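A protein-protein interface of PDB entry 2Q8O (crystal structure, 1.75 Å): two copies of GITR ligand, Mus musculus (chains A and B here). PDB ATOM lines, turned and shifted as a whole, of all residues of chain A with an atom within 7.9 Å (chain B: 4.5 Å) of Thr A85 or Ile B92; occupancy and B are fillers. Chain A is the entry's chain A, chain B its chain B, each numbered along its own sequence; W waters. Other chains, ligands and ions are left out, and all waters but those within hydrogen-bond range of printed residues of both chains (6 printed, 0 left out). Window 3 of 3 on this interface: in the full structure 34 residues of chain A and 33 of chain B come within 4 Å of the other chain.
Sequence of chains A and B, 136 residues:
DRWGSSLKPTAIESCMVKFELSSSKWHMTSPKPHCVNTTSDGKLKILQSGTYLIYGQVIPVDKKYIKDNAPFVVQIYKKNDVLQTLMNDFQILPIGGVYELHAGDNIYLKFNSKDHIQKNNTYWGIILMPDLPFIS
Water W3 bridges the backbone carbonyl oxygen (O) of Thr A85 (2.7 Å) and the side-chain amide oxygen (OE1) of Gln B91 (3.4 Å). Water W2 lies within hydrogen-bond range of the side-chain amide oxygen of Gln B91 (2.7 Å), the backbone NH of Met A87 (3.2 Å) and the backbone carbonyl oxygen of Ile B92 (3.3 Å). Water W5 bridges O of Pro A94 and O of Pro B94. Water W1 bridges the side-chain amide nitrogen of Asn B88 (2.9 Å) and the backbone carbonyl oxygen of Met A87 (2.9 Å). Water W6 bridges OE1 of Gln B57 (2.9 Å) and OH of Tyr A99 (3.2 Å). Water W4 lies within hydrogen-bond range of the side-chain amide oxygen (OE1) of Gln B91 (2.9 Å) and the backbone carbonyl oxygen (O) of Met A87 (3.4 Å).
Hydrophobic or aromatic side chains of chain A that line the printed part of chain B: Leu A86, Met A87, Pro A94 and Tyr A99. Of the 9 printed residues of chain B, 4 touch a printed residue of chain A. Hydrophobic or aromatic side chains of chain B that line the printed part of chain A: Ile B92 and Pro B94. Among the printed residues, 11 pairs touch across the chains. Among the printed residues, no Asp or Glu carboxylate lies within 4 Å of a Lys or Arg side-chain nitrogen of the other chain.
NE2 of Gln B57 touches NE2 of Gln A84 (3.98 Å). CG of Pro B94 touches NE2 of Gln A84 (3.6 Å). Thr A85 touches Ile B92. Leu A86 touches Ile B92 (CD2 to CG2, 3.9 Å). Pro B94 touches Leu A86 (CD to CD2, 3.7 Å). Pro B94 touches Pro A94 (CB to O, 3.7 Å). Gly A96 touches Pro B94. Gln B57 touches Gly A97 (NE2 to CA, 3.7 Å).
O of Met A87 sits close to OE1 of Gln B91. The backbone carbonyl oxygen (O) of Gly A96 sits at hydrogen-bond distance from the side-chain amide nitrogen (NE2) of Gln B57. OH of Tyr A99 sits at hydrogen-bond distance from NE2 of Gln B57, at 3.1 Å.
Leu A83 touches none of the printed residues of chain B. Thr A85 touches just one residue of chain B: Ile B92 (3.7 Å). Printed residues of chain B within 4 Å of Leu A86: Ile B92 (3.9 Å) and Pro B94 (3.7 Å). Printed residues of chain B within 4 Å of Met A87: Gln B91 (3.4 Å). Val B58 touches none of the printed residues of chain A. Of chain A, only Thr A85 (3.7 Å) and Leu A86 (3.9 Å) come within 4 Å of Ile B92.
Pro B94 touches its own counterpart, Pro A94. 2 positions are printed for both chains. Of the 11 pairs that touch across the chains among the printed residues, 1 has its exchanged pair printed and touching as well.
The backbone carbonyl oxygen (O) of Val A74 is in hydrogen-bond range of the backbone NH (N) of Leu A86 (2.8 Å). OG1 of Thr A85 is in hydrogen-bond range of NE2 of Gln A75 (2.8 Å). The backbone NH (N) of Ile A76 lies within hydrogen-bond range of the backbone carbonyl oxygen (O) of Gln A84, 3.0 Å away. OE1 of Gln A84 sits at hydrogen-bond distance from N of Gly A96 (2.9 Å). The side-chain amide nitrogen (NE2) of Gln A84 is in hydrogen-bond range of the side-chain hydroxyl (OH) of Tyr A99, 3.5 Å away. N of Gln B91 lies within hydrogen-bond range of OD1 of Asn B88 (2.9 Å).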
ATOM      1  N   PHE A  72      23.492  32.891 -36.346  1.00  0.00           N
ATOM      2  CA  PHE A  72      23.107  31.570 -36.806  1.00  0.00           C
ATOM      3  C   PHE A  72      22.204  30.928 -35.750  1.00  0.00           C
ATOM      4  O   PHE A  72      22.689  30.492 -34.699  1.00  0.00           O
ATOM      5  CB  PHE A  72      24.395  30.737 -37.020  1.00  0.00           C
ATOM      6  CG  PHE A  72      24.140  29.289 -37.344  1.00  0.00           C
ATOM      7  CD1 PHE A  72      23.244  28.909 -38.351  1.00  0.00           C
ATOM      8  CD2 PHE A  72      24.841  28.295 -36.655  1.00  0.00           C
ATOM      9  CE1 PHE A  72      23.015  27.555 -38.632  1.00  0.00           C
ATOM     10  CE2 PHE A  72      24.639  26.934 -36.939  1.00  0.00           C
ATOM     11  CZ  PHE A  72      23.719  26.560 -37.930  1.00  0.00           C
ATOM     12  N   VAL A  73      20.910  30.854 -36.047  1.00  0.00           N
ATOM     13  CA  VAL A  73      19.909  30.353 -35.088  1.00  0.00           C
ATOM     14  C   VAL A  73      19.006  29.313 -35.738  1.00  0.00           C
ATOM     15  O   VAL A  73      18.542  29.501 -36.859  1.00  0.00           O
ATOM     16  CB  VAL A  73      19.049  31.501 -34.494  1.00  0.00           C
ATOM     17  CG1 VAL A  73      18.105  30.973 -33.344  1.00  0.00           C
ATOM     18  CG2 VAL A  73      19.921  32.657 -33.983  1.00  0.00           C
ATOM     19  N   VAL A  74      18.731  28.223 -35.018  1.00  0.00           N
ATOM     20  CA  VAL A  74      17.789  27.201 -35.497  1.00  0.00           C
ATOM     21  C   VAL A  74      16.754  26.994 -34.411  1.00  0.00           C
ATOM     22  O   VAL A  74      17.121  26.867 -33.233  1.00  0.00           O
ATOM     23  CB  VAL A  74      18.504  25.854 -35.791  1.00  0.00           C
ATOM     24  CG1 VAL A  74      17.485  24.733 -36.163  1.00  0.00           C
ATOM     25  CG2 VAL A  74      19.538  26.063 -36.891  1.00  0.00           C
ATOM     26  N   GLN A  75      15.486  26.952 -34.807  1.00  0.00           N
ATOM     27  CA  GLN A  75      14.403  26.613 -33.885  1.00  0.00           C
ATOM     28  C   GLN A  75      13.639  25.396 -34.387  1.00  0.00           C
ATOM     29  O   GLN A  75      13.384  25.264 -35.574  1.00  0.00           O
ATOM     30  CB  GLN A  75      13.463  27.795 -33.693  1.00  0.00           C
ATOM     31  CG  GLN A  75      14.139  28.928 -32.935  1.00  0.00           C
ATOM     32  CD  GLN A  75      13.202  30.047 -32.640  1.00  0.00           C
ATOM     33  OE1 GLN A  75      12.422  30.454 -33.502  1.00  0.00           O
ATOM     34  NE2 GLN A  75      13.292  30.590 -31.436  1.00  0.00           N
ATOM     35  N   ILE A  76      13.272  24.516 -33.459  1.00  0.00           N
ATOM     36  CA  ILE A  76      12.385  23.410 -33.764  1.00  0.00           C
ATOM     37  C   ILE A  76      11.034  23.785 -33.169  1.00  0.00           C
ATOM     38  O   ILE A  76      10.949  24.213 -32.001  1.00  0.00           O
ATOM     39  CB  ILE A  76      12.830  22.098 -33.122  1.00  0.00           C
ATOM     40  CG1 ILE A  76      14.295  21.800 -33.510  1.00  0.00           C
ATOM     41  CG2 ILE A  76      11.882  20.953 -33.559  1.00  0.00           C
ATOM     42  CD1 ILE A  76      14.874  20.529 -32.840  1.00  0.00           C
ATOM     43  N   TYR A  77       9.994  23.654 -33.983  1.00  0.00           N
ATOM     44  CA  TYR A  77       8.619  23.963 -33.557  1.00  0.00           C
ATOM     45  C   TYR A  77       7.775  22.698 -33.428  1.00  0.00           C
ATOM     46  O   TYR A  77       7.973  21.745 -34.182  1.00  0.00           O
ATOM     47  CB  TYR A  77       7.960  24.843 -34.595  1.00  0.00           C
ATOM     48  CG  TYR A  77       8.367  26.287 -34.489  1.00  0.00           C
ATOM     49  CD1 TYR A  77       9.586  26.733 -35.021  1.00  0.00           C
ATOM     50  CD2 TYR A  77       7.538  27.203 -33.844  1.00  0.00           C
ATOM     51  CE1 TYR A  77       9.960  28.099 -34.929  1.00  0.00           C
ATOM     52  CE2 TYR A  77       7.915  28.570 -33.726  1.00  0.00           C
ATOM     53  CZ  TYR A  77       9.113  28.988 -34.269  1.00  0.00           C
ATOM     54  OH  TYR A  77       9.470  30.319 -34.145  1.00  0.00           O
ATOM     55  N   VAL A  82       7.489  26.957 -29.788  1.00  0.00           N
ATOM     56  CA  VAL A  82       8.929  26.673 -29.924  1.00  0.00           C
ATOM     57  C   VAL A  82       9.335  25.552 -28.959  1.00  0.00           C
ATOM     58  O   VAL A  82       9.130  25.674 -27.738  1.00  0.00           O
ATOM     59  CB  VAL A  82       9.784  27.936 -29.655  1.00  0.00           C
ATOM     60  CG1 VAL A  82      11.294  27.608 -29.789  1.00  0.00           C
ATOM     61  CG2 VAL A  82       9.369  29.064 -30.575  1.00  0.00           C
ATOM     62  N   LEU A  83       9.903  24.482 -29.507  1.00  0.00           N
ATOM     63  CA  LEU A  83      10.374  23.354 -28.716  1.00  0.00           C
ATOM     64  C   LEU A  83      11.809  23.556 -28.222  1.00  0.00           C
ATOM     65  O   LEU A  83      12.186  23.106 -27.135  1.00  0.00           O
ATOM     66  CB  LEU A  83      10.296  22.095 -29.573  1.00  0.00           C
ATOM     67  CG  LEU A  83      10.088  20.721 -28.963  1.00  0.00           C
ATOM     68  CD1 LEU A  83       8.842  20.668 -28.058  1.00  0.00           C
ATOM     69  CD2 LEU A  83       9.978  19.740 -30.110  1.00  0.00           C
ATOM     70  N   GLN A  84      12.631  24.203 -29.039  1.00  0.00           N
ATOM     71  CA  GLN A  84      13.999  24.554 -28.681  1.00  0.00           C
ATOM     72  C   GLN A  84      14.565  25.608 -29.625  1.00  0.00           C
ATOM     73  O   GLN A  84      14.130  25.682 -30.785  1.00  0.00           O
ATOM     74  CB  GLN A  84      14.890  23.310 -28.688  1.00  0.00           C
ATOM     75  CG  GLN A  84      15.328  22.867 -30.073  1.00  0.00           C
ATOM     76  CD  GLN A  84      16.452  21.850 -30.033  1.00  0.00           C
ATOM     77  OE1 GLN A  84      17.132  21.629 -31.036  1.00  0.00           O
ATOM     78  NE2 GLN A  84      16.650  21.229 -28.874  1.00  0.00           N
ATOM     79  N   THR A  85      15.442  26.421 -29.069  1.00  0.00           N
ATOM     80  CA  THR A  85      16.125  27.451 -29.799  1.00  0.00           C
ATOM     81  C   THR A  85      17.617  27.218 -29.588  1.00  0.00           C
ATOM     82  O   THR A  85      18.080  27.131 -28.442  1.00  0.00           O
ATOM     83  CB  THR A  85      15.742  28.866 -29.283  1.00  0.00           C
ATOM     84  OG1 THR A  85      14.323  29.041 -29.372  1.00  0.00           O
ATOM     85  CG2 THR A  85      16.402  29.918 -30.126  1.00  0.00           C
ATOM     86  N   LEU A  86      18.362  27.157 -30.689  1.00  0.00           N
ATOM     87  CA  LEU A  86      19.788  26.834 -30.657  1.00  0.00           C
ATOM     88  C   LEU A  86      20.546  27.882 -31.424  1.00  0.00           C
ATOM     89  O   LEU A  86      20.084  28.352 -32.478  1.00  0.00           O
ATOM     90  CB  LEU A  86      20.016  25.494 -31.365  1.00  0.00           C
ATOM     91  CG  LEU A  86      19.173  24.321 -30.839  1.00  0.00           C
ATOM     92  CD1 LEU A  86      19.479  23.064 -31.638  1.00  0.00           C
ATOM     93  CD2 LEU A  86      19.396  24.115 -29.348  1.00  0.00           C
ATOM     94  N   MET A  87      21.715  28.226 -30.920  1.00  0.00           N
ATOM     95  CA  MET A  87      22.587  29.130 -31.658  1.00  0.00           C
ATOM     96  C   MET A  87      24.023  28.869 -31.317  1.00  0.00           C
ATOM     97  O   MET A  87      24.350  28.481 -30.186  1.00  0.00           O
ATOM     98  CB  MET A  87      22.204  30.598 -31.464  1.00  0.00           C
ATOM     99  CG  MET A  87      22.172  31.103 -30.081  1.00  0.00           C
ATOM    100  SD  MET A  87      21.723  32.856 -30.161  1.00  0.00           S
ATOM    101  CE  MET A  87      19.959  32.711 -29.866  1.00  0.00           C
ATOM    102  N   LEU A  93      25.871  21.971 -35.967  1.00  0.00           N
ATOM    103  CA  LEU A  93      24.875  22.175 -34.920  1.00  0.00           C
ATOM    104  C   LEU A  93      23.962  20.943 -34.762  1.00  0.00           C
ATOM    105  O   LEU A  93      22.986  20.803 -35.496  1.00  0.00           O
ATOM    106  CB  LEU A  93      24.067  23.443 -35.270  1.00  0.00           C
ATOM    107  CG  LEU A  93      23.275  24.296 -34.263  1.00  0.00           C
ATOM    108  CD1 LEU A  93      21.777  23.972 -34.312  1.00  0.00           C
ATOM    109  CD2 LEU A  93      23.835  24.245 -32.839  1.00  0.00           C
ATOM    110  N   PRO A  94      24.298  20.024 -33.827  1.00  0.00           N
ATOM    111  CA  PRO A  94      23.390  18.923 -33.526  1.00  0.00           C
ATOM    112  C   PRO A  94      22.099  19.512 -32.929  1.00  0.00           C
ATOM    113  O   PRO A  94      22.168  20.537 -32.238  1.00  0.00           O
ATOM    114  CB  PRO A  94      24.158  18.085 -32.478  1.00  0.00           C
ATOM    115  CG  PRO A  94      25.610  18.452 -32.674  1.00  0.00           C
ATOM    116  CD  PRO A  94      25.544  19.945 -33.024  1.00  0.00           C
ATOM    117  N   GLY A  96      17.807  18.779 -31.367  1.00  0.00           N
ATOM    118  CA  GLY A  96      16.769  17.840 -30.918  1.00  0.00           C
ATOM    119  C   GLY A  96      16.943  17.323 -29.491  1.00  0.00           C
ATOM    120  O   GLY A  96      17.477  18.019 -28.598  1.00  0.00           O
ATOM    121  N   GLY A  97      16.459  16.110 -29.265  1.00  0.00           N
ATOM    122  CA  GLY A  97      16.298  15.589 -27.897  1.00  0.00           C
ATOM    123  C   GLY A  97      15.024  14.757 -27.793  1.00  0.00           C
ATOM    124  O   GLY A  97      14.336  14.540 -28.797  1.00  0.00           O
ATOM    125  N   TYR A  99      11.310  14.144 -26.680  1.00  0.00           N
ATOM    126  CA  TYR A  99      10.088  14.923 -26.471  1.00  0.00           C
ATOM    127  C   TYR A  99       8.849  14.043 -26.506  1.00  0.00           C
ATOM    128  O   TYR A  99       8.752  13.128 -27.293  1.00  0.00           O
ATOM    129  CB  TYR A  99       9.957  16.040 -27.522  1.00  0.00           C
ATOM    130  CG  TYR A  99      11.066  17.055 -27.405  1.00  0.00           C
ATOM    131  CD1 TYR A  99      12.239  16.944 -28.150  1.00  0.00           C
ATOM    132  CD2 TYR A  99      10.959  18.096 -26.485  1.00  0.00           C
ATOM    133  CE1 TYR A  99      13.277  17.888 -28.002  1.00  0.00           C
ATOM    134  CE2 TYR A  99      11.959  19.044 -26.343  1.00  0.00           C
ATOM    135  CZ  TYR A  99      13.123  18.917 -27.088  1.00  0.00           C
ATOM    136  OH  TYR A  99      14.126  19.849 -26.922  1.00  0.00           O
ATOM    137  N   LYS A 110      12.846  26.136 -38.333  1.00  0.00           N
ATOM    138  CA  LYS A 110      12.914  27.489 -38.865  1.00  0.00           C
ATOM    139  C   LYS A 110      14.330  27.986 -38.605  1.00  0.00           C
ATOM    140  O   LYS A 110      14.944  27.684 -37.561  1.00  0.00           O
ATOM    141  CB  LYS A 110      11.901  28.398 -38.171  1.00  0.00           C
ATOM    142  CG  LYS A 110      10.446  28.000 -38.497  1.00  0.00           C
ATOM    143  CD  LYS A 110       9.865  28.768 -39.683  1.00  0.00           C
ATOM    144  CE  LYS A 110       9.173  30.035 -39.212  1.00  0.00           C
ATOM    145  NZ  LYS A 110       8.643  29.929 -37.801  1.00  0.00           N
ATOM    146  N   GLN B  57      21.128  15.758 -24.225  1.00  0.00           N
ATOM    147  CA  GLN B  57      21.157  17.206 -24.009  1.00  0.00           C
ATOM    148  C   GLN B  57      21.989  17.470 -22.785  1.00  0.00           C
ATOM    149  O   GLN B  57      21.769  16.835 -21.758  1.00  0.00           O
ATOM    150  CB  GLN B  57      19.752  17.784 -23.795  1.00  0.00           C
ATOM    151  CG  GLN B  57      18.834  17.710 -25.016  1.00  0.00           C
ATOM    152  CD  GLN B  57      17.493  18.403 -24.785  1.00  0.00           C
ATOM    153  OE1 GLN B  57      17.135  18.735 -23.648  1.00  0.00           O
ATOM    154  NE2 GLN B  57      16.741  18.623 -25.870  1.00  0.00           N
ATOM    155  N   VAL B  58      22.952  18.386 -22.934  1.00  0.00           N
ATOM    156  CA  VAL B  58      23.717  18.917 -21.818  1.00  0.00           C
ATOM    157  C   VAL B  58      23.166  20.292 -21.464  1.00  0.00           C
ATOM    158  O   VAL B  58      23.201  21.241 -22.271  1.00  0.00           O
ATOM    159  CB  VAL B  58      25.230  18.938 -22.098  1.00  0.00           C
ATOM    160  CG1 VAL B  58      26.000  19.442 -20.845  1.00  0.00           C
ATOM    161  CG2 VAL B  58      25.678  17.492 -22.510  1.00  0.00           C
ATOM    162  N   ILE B  59      22.634  20.369 -20.251  1.00  0.00           N
ATOM    163  CA  ILE B  59      22.075  21.619 -19.733  1.00  0.00           C
ATOM    164  C   ILE B  59      23.096  22.331 -18.840  1.00  0.00           C
ATOM    165  O   ILE B  59      23.527  21.788 -17.826  1.00  0.00           O
ATOM    166  CB  ILE B  59      20.778  21.389 -18.931  1.00  0.00           C
ATOM    167  CG1 ILE B  59      19.753  20.531 -19.713  1.00  0.00           C
ATOM    168  CG2 ILE B  59      20.167  22.728 -18.487  1.00  0.00           C
ATOM    169  CD1 ILE B  59      19.413  21.062 -21.085  1.00  0.00           C
ATOM    170  N   PRO B  60      23.507  23.553 -19.238  1.00  0.00           N
ATOM    171  CA  PRO B  60      24.421  24.304 -18.359  1.00  0.00           C
ATOM    172  C   PRO B  60      23.729  24.988 -17.165  1.00  0.00           C
ATOM    173  O   PRO B  60      22.527  25.292 -17.210  1.00  0.00           O
ATOM    174  CB  PRO B  60      25.017  25.366 -19.294  1.00  0.00           C
ATOM    175  CG  PRO B  60      23.929  25.640 -20.288  1.00  0.00           C
ATOM    176  CD  PRO B  60      23.207  24.280 -20.488  1.00  0.00           C
ATOM    177  N   ASN B  88      29.388  26.429 -26.752  1.00  0.00           N
ATOM    178  CA  ASN B  88      28.565  27.627 -26.874  1.00  0.00           C
ATOM    179  C   ASN B  88      28.674  28.473 -25.605  1.00  0.00           C
ATOM    180  O   ASN B  88      29.432  28.125 -24.684  1.00  0.00           O
ATOM    181  CB  ASN B  88      27.105  27.259 -27.240  1.00  0.00           C
ATOM    182  CG  ASN B  88      26.336  26.584 -26.103  1.00  0.00           C
ATOM    183  OD1 ASN B  88      26.645  26.755 -24.924  1.00  0.00           O
ATOM    184  ND2 ASN B  88      25.296  25.845 -26.465  1.00  0.00           N
ATOM    185  N   GLN B  91      24.606  27.623 -23.059  1.00  0.00           N
ATOM    186  CA  GLN B  91      23.224  27.450 -23.492  1.00  0.00           C
ATOM    187  C   GLN B  91      22.943  25.970 -23.708  1.00  0.00           C
ATOM    188  O   GLN B  91      23.876  25.151 -23.849  1.00  0.00           O
ATOM    189  CB  GLN B  91      22.988  28.170 -24.828  1.00  0.00           C
ATOM    190  CG  GLN B  91      23.120  29.668 -24.819  1.00  0.00           C
ATOM    191  CD  GLN B  91      22.936  30.226 -26.230  1.00  0.00           C
ATOM    192  OE1 GLN B  91      23.120  29.506 -27.223  1.00  0.00           O
ATOM    193  NE2 GLN B  91      22.586  31.504 -26.328  1.00  0.00           N
ATOM    194  N   ILE B  92      21.654  25.637 -23.787  1.00  0.00           N
ATOM    195  CA  ILE B  92      21.219  24.255 -24.068  1.00  0.00           C
ATOM    196  C   ILE B  92      22.012  23.639 -25.211  1.00  0.00           C
ATOM    197  O   ILE B  92      22.185  24.251 -26.270  1.00  0.00           O
ATOM    198  CB  ILE B  92      19.680  24.186 -24.384  1.00  0.00           C
ATOM    199  CG1 ILE B  92      19.266  22.714 -24.578  1.00  0.00           C
ATOM    200  CG2 ILE B  92      19.281  25.136 -25.574  1.00  0.00           C
ATOM    201  CD1 ILE B  92      17.780  22.504 -24.945  1.00  0.00           C
ATOM    202  N   LEU B  93      22.445  22.396 -25.015  1.00  0.00           N
ATOM    203  CA  LEU B  93      23.395  21.777 -25.924  1.00  0.00           C
ATOM    204  C   LEU B  93      22.983  20.343 -26.277  1.00  0.00           C
ATOM    205  O   LEU B  93      23.450  19.397 -25.639  1.00  0.00           O
ATOM    206  CB  LEU B  93      24.777  21.808 -25.252  1.00  0.00           C
ATOM    207  CG  LEU B  93      26.143  21.923 -25.937  1.00  0.00           C
ATOM    208  CD1 LEU B  93      26.763  20.537 -26.098  1.00  0.00           C
ATOM    209  CD2 LEU B  93      26.159  22.738 -27.247  1.00  0.00           C
ATOM    210  N   PRO B  94      22.099  20.175 -27.297  1.00  0.00           N
ATOM    211  CA  PRO B  94      21.842  18.841 -27.873  1.00  0.00           C
ATOM    212  C   PRO B  94      23.174  18.338 -28.428  1.00  0.00           C
ATOM    213  O   PRO B  94      23.999  19.146 -28.877  1.00  0.00           O
ATOM    214  CB  PRO B  94      20.852  19.133 -29.025  1.00  0.00           C
ATOM    215  CG  PRO B  94      20.159  20.444 -28.581  1.00  0.00           C
ATOM    216  CD  PRO B  94      21.318  21.223 -27.977  1.00  0.00           C
HETATM  217  O   HOH W   1      24.925  25.741 -29.320  1.00  0.00           O
HETATM  218  O   HOH W   2      22.107  27.083 -27.980  1.00  0.00           O
HETATM  219  O   HOH W   3      19.763  28.781 -27.151  1.00  0.00           O
HETATM  220  O   HOH W   4      25.921  30.269 -27.709  1.00  0.00           O
HETATM  221  O   HOH W   5      23.916  21.566 -30.304  1.00  0.00           O
HETATM  222  O   HOH W   6      14.310  19.394 -23.743  1.00  0.00           O
